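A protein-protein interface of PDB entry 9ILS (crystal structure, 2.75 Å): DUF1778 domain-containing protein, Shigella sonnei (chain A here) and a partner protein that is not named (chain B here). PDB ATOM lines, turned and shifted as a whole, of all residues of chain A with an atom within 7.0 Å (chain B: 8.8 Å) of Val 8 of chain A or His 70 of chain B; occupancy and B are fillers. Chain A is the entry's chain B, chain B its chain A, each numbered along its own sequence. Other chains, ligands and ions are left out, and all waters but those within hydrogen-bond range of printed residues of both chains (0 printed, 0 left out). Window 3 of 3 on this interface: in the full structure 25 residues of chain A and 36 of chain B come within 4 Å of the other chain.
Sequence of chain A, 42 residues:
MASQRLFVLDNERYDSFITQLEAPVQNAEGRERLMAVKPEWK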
ATOM      1  N   GLN A   4      34.767 -14.443 -13.351  1.00  0.00           N
ATOM      2  CA  GLN A   4      33.695 -14.502 -14.344  1.00  0.00           C
ATOM      3  C   GLN A   4      34.179 -14.720 -15.788  1.00  0.00           C
ATOM      4  O   GLN A   4      35.084 -14.014 -16.254  1.00  0.00           O
ATOM      5  CB  GLN A   4      32.894 -13.214 -14.314  1.00  0.00           C
ATOM      6  CG  GLN A   4      31.700 -13.207 -15.251  1.00  0.00           C
ATOM      7  CD  GLN A   4      31.067 -11.823 -15.350  1.00  0.00           C
ATOM      8  OE1 GLN A   4      30.012 -11.642 -15.979  1.00  0.00           O
ATOM      9  NE2 GLN A   4      31.741 -10.823 -14.769  1.00  0.00           N
ATOM     10  N   LEU A   6      31.487 -15.957 -18.476  1.00  0.00           N
ATOM     11  CA  LEU A   6      30.364 -16.006 -19.429  1.00  0.00           C
ATOM     12  C   LEU A   6      29.418 -14.863 -19.087  1.00  0.00           C
ATOM     13  O   LEU A   6      28.672 -14.939 -18.110  1.00  0.00           O
ATOM     14  CB  LEU A   6      29.635 -17.351 -19.422  1.00  0.00           C
ATOM     15  CG  LEU A   6      28.268 -17.502 -20.123  1.00  0.00           C
ATOM     16  CD1 LEU A   6      28.370 -17.814 -21.613  1.00  0.00           C
ATOM     17  CD2 LEU A   6      27.400 -18.564 -19.431  1.00  0.00           C
ATOM     18  N   PHE A   7      29.455 -13.805 -19.888  1.00  0.00           N
ATOM     19  CA  PHE A   7      28.640 -12.630 -19.628  1.00  0.00           C
ATOM     20  C   PHE A   7      27.285 -12.850 -20.290  1.00  0.00           C
ATOM     21  O   PHE A   7      27.187 -12.941 -21.520  1.00  0.00           O
ATOM     22  CB  PHE A   7      29.339 -11.375 -20.133  1.00  0.00           C
ATOM     23  CG  PHE A   7      30.674 -11.126 -19.483  1.00  0.00           C
ATOM     24  CD1 PHE A   7      31.785 -11.848 -19.853  1.00  0.00           C
ATOM     25  CD2 PHE A   7      30.813 -10.176 -18.488  1.00  0.00           C
ATOM     26  CE1 PHE A   7      33.023 -11.615 -19.248  1.00  0.00           C
ATOM     27  CE2 PHE A   7      32.051  -9.939 -17.876  1.00  0.00           C
ATOM     28  CZ  PHE A   7      33.151 -10.661 -18.257  1.00  0.00           C
ATOM     29  N   VAL A   8      26.249 -12.996 -19.474  1.00  0.00           N
ATOM     30  CA  VAL A   8      24.890 -13.153 -19.968  1.00  0.00           C
ATOM     31  C   VAL A   8      24.194 -11.819 -19.776  1.00  0.00           C
ATOM     32  O   VAL A   8      24.205 -11.253 -18.675  1.00  0.00           O
ATOM     33  CB  VAL A   8      24.153 -14.289 -19.253  1.00  0.00           C
ATOM     34  CG1 VAL A   8      22.999 -14.773 -20.119  1.00  0.00           C
ATOM     35  CG2 VAL A   8      25.118 -15.413 -18.964  1.00  0.00           C
ATOM     36  N   LEU A   9      23.629 -11.297 -20.854  1.00  0.00           N
ATOM     37  CA  LEU A   9      23.125  -9.939 -20.868  1.00  0.00           C
ATOM     38  C   LEU A   9      21.690  -9.944 -21.368  1.00  0.00           C
ATOM     39  O   LEU A   9      21.318 -10.751 -22.227  1.00  0.00           O
ATOM     40  CB  LEU A   9      24.000  -9.042 -21.753  1.00  0.00           C
ATOM     41  CG  LEU A   9      25.409  -8.784 -21.221  1.00  0.00           C
ATOM     42  CD1 LEU A   9      26.005  -7.583 -21.918  1.00  0.00           C
ATOM     43  CD2 LEU A   9      25.446  -8.592 -19.706  1.00  0.00           C
ATOM     44  N   ASP A  10      20.886  -9.042 -20.801  1.00  0.00           N
ATOM     45  CA  ASP A  10      19.559  -8.764 -21.330  1.00  0.00           C
ATOM     46  C   ASP A  10      19.668  -8.333 -22.796  1.00  0.00           C
ATOM     47  O   ASP A  10      20.757  -8.034 -23.307  1.00  0.00           O
ATOM     48  CB  ASP A  10      18.858  -7.719 -20.454  1.00  0.00           C
ATOM     49  CG  ASP A  10      19.409  -6.289 -20.637  1.00  0.00           C
ATOM     50  OD1 ASP A  10      19.704  -5.641 -19.604  1.00  0.00           O
ATOM     51  OD2 ASP A  10      19.506  -5.785 -21.784  1.00  0.00           O
ATOM     52  N   ASN A  11      18.522  -8.286 -23.479  1.00  0.00           N
ATOM     53  CA  ASN A  11      18.532  -8.050 -24.923  1.00  0.00           C
ATOM     54  C   ASN A  11      19.139  -6.701 -25.274  1.00  0.00           C
ATOM     55  O   ASN A  11      19.847  -6.569 -26.282  1.00  0.00           O
ATOM     56  CB  ASN A  11      17.117  -8.138 -25.470  1.00  0.00           C
ATOM     57  CG  ASN A  11      16.810  -9.495 -26.034  1.00  0.00           C
ATOM     58  OD1 ASN A  11      17.102 -10.519 -25.413  1.00  0.00           O
ATOM     59  ND2 ASN A  11      16.207  -9.516 -27.227  1.00  0.00           N
ATOM     60  N   ARG A  13      21.269  -4.618 -23.325  1.00  0.00           N
ATOM     61  CA  ARG A  13      22.710  -4.611 -23.102  1.00  0.00           C
ATOM     62  C   ARG A  13      23.428  -5.396 -24.195  1.00  0.00           C
ATOM     63  O   ARG A  13      24.510  -4.991 -24.644  1.00  0.00           O
ATOM     64  CB  ARG A  13      23.055  -5.171 -21.711  1.00  0.00           C
ATOM     65  CG  ARG A  13      23.148  -4.132 -20.576  1.00  0.00           C
ATOM     66  CD  ARG A  13      23.581  -4.783 -19.251  1.00  0.00           C
ATOM     67  NE  ARG A  13      22.633  -4.484 -18.179  1.00  0.00           N
ATOM     68  CZ  ARG A  13      21.802  -5.372 -17.643  1.00  0.00           C
ATOM     69  NH1 ARG A  13      21.826  -6.647 -18.007  1.00  0.00           N
ATOM     70  NH2 ARG A  13      20.905  -4.965 -16.745  1.00  0.00           N
ATOM     71  N   TYR A  14      22.824  -6.489 -24.678  1.00  0.00           N
ATOM     72  CA  TYR A  14      23.498  -7.289 -25.697  1.00  0.00           C
ATOM     73  C   TYR A  14      23.646  -6.515 -27.006  1.00  0.00           C
ATOM     74  O   TYR A  14      24.724  -6.523 -27.611  1.00  0.00           O
ATOM     75  CB  TYR A  14      22.757  -8.612 -25.929  1.00  0.00           C
ATOM     76  CG  TYR A  14      23.493  -9.559 -26.869  1.00  0.00           C
ATOM     77  CD1 TYR A  14      24.635 -10.254 -26.461  1.00  0.00           C
ATOM     78  CD2 TYR A  14      23.058  -9.737 -28.177  1.00  0.00           C
ATOM     79  CE1 TYR A  14      25.301 -11.116 -27.340  1.00  0.00           C
ATOM     80  CE2 TYR A  14      23.709 -10.597 -29.043  1.00  0.00           C
ATOM     81  CZ  TYR A  14      24.820 -11.278 -28.625  1.00  0.00           C
ATOM     82  OH  TYR A  14      25.445 -12.112 -29.519  1.00  0.00           O
ATOM     83  N   ASP A  15      22.592  -5.817 -27.447  1.00  0.00           N
ATOM     84  CA  ASP A  15      22.704  -5.005 -28.661  1.00  0.00           C
ATOM     85  C   ASP A  15      23.704  -3.864 -28.490  1.00  0.00           C
ATOM     86  O   ASP A  15      24.444  -3.543 -29.427  1.00  0.00           O
ATOM     87  CB  ASP A  15      21.329  -4.472 -29.062  1.00  0.00           C
ATOM     88  CG  ASP A  15      20.304  -5.575 -29.201  1.00  0.00           C
ATOM     89  OD1 ASP A  15      20.705  -6.717 -29.483  1.00  0.00           O
ATOM     90  OD2 ASP A  15      19.107  -5.326 -28.974  1.00  0.00           O
ATOM     91  N   SER B  67      32.769 -15.974 -23.175  1.00  0.00           N
ATOM     92  CA  SER B  67      31.740 -15.769 -24.185  1.00  0.00           C
ATOM     93  C   SER B  67      30.758 -14.723 -23.671  1.00  0.00           C
ATOM     94  O   SER B  67      30.719 -14.413 -22.476  1.00  0.00           O
ATOM     95  CB  SER B  67      31.054 -17.096 -24.535  1.00  0.00           C
ATOM     96  OG  SER B  67      29.933 -16.906 -25.372  1.00  0.00           O
ATOM     97  N   VAL B  68      30.010 -14.133 -24.602  1.00  0.00           N
ATOM     98  CA  VAL B  68      28.953 -13.178 -24.288  1.00  0.00           C
ATOM     99  C   VAL B  68      27.732 -13.593 -25.085  1.00  0.00           C
ATOM    100  O   VAL B  68      27.826 -13.806 -26.300  1.00  0.00           O
ATOM    101  CB  VAL B  68      29.341 -11.720 -24.619  1.00  0.00           C
ATOM    102  CG1 VAL B  68      28.303 -10.736 -24.064  1.00  0.00           C
ATOM    103  CG2 VAL B  68      30.742 -11.382 -24.103  1.00  0.00           C
ATOM    104  N   THR B  69      26.595 -13.737 -24.406  1.00  0.00           N
ATOM    105  CA  THR B  69      25.365 -14.138 -25.077  1.00  0.00           C
ATOM    106  C   THR B  69      24.208 -13.378 -24.438  1.00  0.00           C
ATOM    107  O   THR B  69      24.389 -12.647 -23.458  1.00  0.00           O
ATOM    108  CB  THR B  69      25.192 -15.664 -25.018  1.00  0.00           C
ATOM    109  OG1 THR B  69      24.140 -16.072 -25.904  1.00  0.00           O
ATOM    110  CG2 THR B  69      24.873 -16.125 -23.598  1.00  0.00           C
ATOM    111  N   HIS B  70      23.020 -13.520 -25.017  1.00  0.00           N
ATOM    112  CA  HIS B  70      21.810 -12.946 -24.449  1.00  0.00           C
ATOM    113  C   HIS B  70      21.059 -14.003 -23.658  1.00  0.00           C
ATOM    114  O   HIS B  70      21.400 -15.190 -23.661  1.00  0.00           O
ATOM    115  CB  HIS B  70      20.914 -12.395 -25.546  1.00  0.00           C
ATOM    116  CG  HIS B  70      20.920 -13.245 -26.771  1.00  0.00           C
ATOM    117  ND1 HIS B  70      20.721 -14.611 -26.725  1.00  0.00           N
ATOM    118  CD2 HIS B  70      21.150 -12.941 -28.071  1.00  0.00           C
ATOM    119  CE1 HIS B  70      20.798 -15.105 -27.949  1.00  0.00           C
ATOM    120  NE2 HIS B  70      21.063 -14.114 -28.784  1.00  0.00           N
ATOM    121  N   ALA B  71      20.002 -13.564 -22.999  1.00  0.00           N
ATOM    122  CA  ALA B  71      19.107 -14.463 -22.283  1.00  0.00           C
ATOM    123  C   ALA B  71      17.950 -14.770 -23.223  1.00  0.00           C
ATOM    124  O   ALA B  71      17.029 -13.960 -23.363  1.00  0.00           O
ATOM    125  CB  ALA B  71      18.632 -13.828 -20.985  1.00  0.00           C
ATOM    126  N   GLU B  72      18.024 -15.932 -23.883  1.00  0.00           N
ATOM    127  CA  GLU B  72      16.999 -16.398 -24.816  1.00  0.00           C
ATOM    128  C   GLU B  72      16.299 -15.267 -25.595  1.00  0.00           C
ATOM    129  O   GLU B  72      16.419 -15.152 -26.811  1.00  0.00           O
ATOM    130  CB  GLU B  72      15.965 -17.213 -24.052  1.00  0.00           C
ATOM    131  CG  GLU B  72      14.611 -17.300 -24.729  1.00  0.00           C
ATOM    132  CD  GLU B  72      13.449 -17.254 -23.741  1.00  0.00           C
ATOM    133  OE1 GLU B  72      12.696 -16.251 -23.759  1.00  0.00           O
ATOM    134  OE2 GLU B  72      13.308 -18.227 -22.939  1.00  0.00           O
ATOM    135  N   PRO B  82      29.128 -14.776 -33.589  1.00  0.00           N
ATOM    136  CA  PRO B  82      27.739 -14.336 -33.685  1.00  0.00           C
ATOM    137  C   PRO B  82      27.007 -14.538 -32.370  1.00  0.00           C
ATOM    138  O   PRO B  82      27.275 -13.763 -31.453  1.00  0.00           O
ATOM    139  CB  PRO B  82      27.154 -15.232 -34.780  1.00  0.00           C
ATOM    140  CG  PRO B  82      28.319 -15.621 -35.609  1.00  0.00           C
ATOM    141  CD  PRO B  82      29.463 -15.745 -34.643  1.00  0.00           C
ATOM    142  N   ASN B  83      26.148 -15.569 -32.270  1.00  0.00           N
ATOM    143  CA  ASN B  83      25.216 -15.717 -31.143  1.00  0.00           C
ATOM    144  C   ASN B  83      25.912 -15.747 -29.783  1.00  0.00           C
ATOM    145  O   ASN B  83      25.548 -14.943 -28.908  1.00  0.00           O
ATOM    146  CB  ASN B  83      24.332 -16.963 -31.358  1.00  0.00           C
ATOM    147  CG  ASN B  83      23.428 -17.283 -30.143  1.00  0.00           C
ATOM    148  OD1 ASN B  83      22.369 -16.679 -29.975  1.00  0.00           O
ATOM    149  ND2 ASN B  83      23.843 -18.246 -29.309  1.00  0.00           N
ATOM    150  N   PRO B  84      26.863 -16.630 -29.520  1.00  0.00           N
ATOM    151  CA  PRO B  84      27.806 -16.330 -28.440  1.00  0.00           C
ATOM    152  C   PRO B  84      29.006 -15.622 -29.039  1.00  0.00           C
ATOM    153  O   PRO B  84      29.501 -15.977 -30.111  1.00  0.00           O
ATOM    154  CB  PRO B  84      28.143 -17.712 -27.860  1.00  0.00           C
ATOM    155  CG  PRO B  84      27.405 -18.719 -28.732  1.00  0.00           C
ATOM    156  CD  PRO B  84      27.004 -18.019 -29.978  1.00  0.00           C
ATOM    157  N   VAL B  85      29.456 -14.555 -28.396  1.00  0.00           N
ATOM    158  CA  VAL B  85      30.543 -13.746 -28.932  1.00  0.00           C
ATOM    159  C   VAL B  85      31.851 -14.274 -28.333  1.00  0.00           C
ATOM    160  O   VAL B  85      32.010 -14.243 -27.109  1.00  0.00           O
ATOM    161  CB  VAL B  85      30.330 -12.265 -28.620  1.00  0.00           C
ATOM    162  CG1 VAL B  85      31.246 -11.435 -29.449  1.00  0.00           C
ATOM    163  CG2 VAL B  85      28.884 -11.877 -28.923  1.00  0.00           C
ATOM    164  N   VAL B 150      29.975  -2.259 -22.100  1.00  0.00           N
ATOM    165  CA  VAL B 150      28.675  -2.310 -21.443  1.00  0.00           C
ATOM    166  C   VAL B 150      28.499  -3.551 -20.568  1.00  0.00           C
ATOM    167  O   VAL B 150      27.536  -3.603 -19.790  1.00  0.00           O
ATOM    168  CB  VAL B 150      27.535  -2.247 -22.480  1.00  0.00           C
ATOM    169  CG1 VAL B 150      26.209  -1.863 -21.804  1.00  0.00           C
ATOM    170  CG2 VAL B 150      27.869  -1.286 -23.608  1.00  0.00           C
ATOM    171  N   VAL B 151      29.386  -4.551 -20.680  1.00  0.00           N
ATOM    172  CA  VAL B 151      29.220  -5.787 -19.911  1.00  0.00           C
ATOM    173  C   VAL B 151      29.195  -5.482 -18.411  1.00  0.00           C
ATOM    174  O   VAL B 151      28.282  -5.903 -17.688  1.00  0.00           O
ATOM    175  CB  VAL B 151      30.311  -6.817 -20.280  1.00  0.00           C
ATOM    176  CG1 VAL B 151      29.718  -7.978 -21.065  1.00  0.00           C
ATOM    177  CG2 VAL B 151      31.399  -6.179 -21.102  1.00  0.00           C
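OH of Tyr 14 of chain A sits at hydrogen-bond distance from O of Asn 83 of chain B (2.9 Å). O of Pro 82 of chain B sits at hydrogen-bond distance from OH of Tyr 14 of chain A, 3.1 Å away. The backbone NH of Leu 9 of chain A lies within hydrogen-bond range of the backbone carbonyl oxygen of Thr 69 of chain B (3.0 Å). O of Phe 7 of chain A sits at hydrogen-bond distance from N of Thr 69 of chain B, at 3.1 Å. The backbone carbonyl oxygen (O) of Ser 67 of chain B is in hydrogen-bond range of the backbone NH (N) of Phe 7 of chain A (2.9 Å). The backbone NH (N) of Ala 71 of chain B is in hydrogen-bond range of the backbone carbonyl oxygen (O) of Leu 9 of chain A.
Along chain B the printed residues that touch a printed residue of chain A span positions 67 to 151. Of the 10 printed residues of chain A, 5 touch a printed residue of chain B. Hydrophobic or aromatic side chains of chain A that line the printed part of chain B: Phe 7, Val 8, Leu 9 and Tyr 14.
Val 8 of chain A touches two residues of chain B. His 70 of chain B touches three residues of chain A. Of the printed residues of chain B, Leu 9 of chain A touches Thr 69, His 70, Ala 71 and Val 151. Of the printed residues of chain B, Tyr 14 of chain A touches Val 68, Thr 69, His 70, Pro 82, Asn 83 and Val 85. Printed residues of chain A within 4 Å of Val 68 of chain B: Phe 7 (3.3 Å) and Tyr 14 (3.8 Å). Gln 4 of chain A touches none of the printed residues of chain B. The nearest residue of chain B that does not touch Val 8 of chain A is Ala 71 of chain B (4.3 Å). The nearest residue of chain A that does not touch His 70 of chain B is Asn 11 of chain A (4.3 Å).
A ring nitrogen (NE2) of His 70 of chain B sits close to the side-chain amide oxygen (OD1) of Asn 83 of chain B (3.1 Å). The backbone carbonyl oxygen (O) of Val 68 of chain B lies within hydrogen-bond range of the backbone NH (N) of Val 85 of chain B (2.8 Å).
Among the printed residues, merely in contact across the chains: Leu 9 of chain A with His 70 of chain B, Phe 7 of chain A with Val 68 of chain B, Leu 6 of chain A with Ser 67 of chain B, Tyr 14 of chain A with Val 85 of chain B, Phe 7 of chain A with Val 151 of chain B, Val 8 of chain A with Thr 69 of chain B, Tyr 14 of chain A with His 70 of chain B, Tyr 14 of chain A with Thr 69 of chain B, Leu 9 of chain A with Val 151 of chain B, Tyr 14 of chain A with Val 68 of chain B and Val 8 of chain A with His 70 of chain B.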
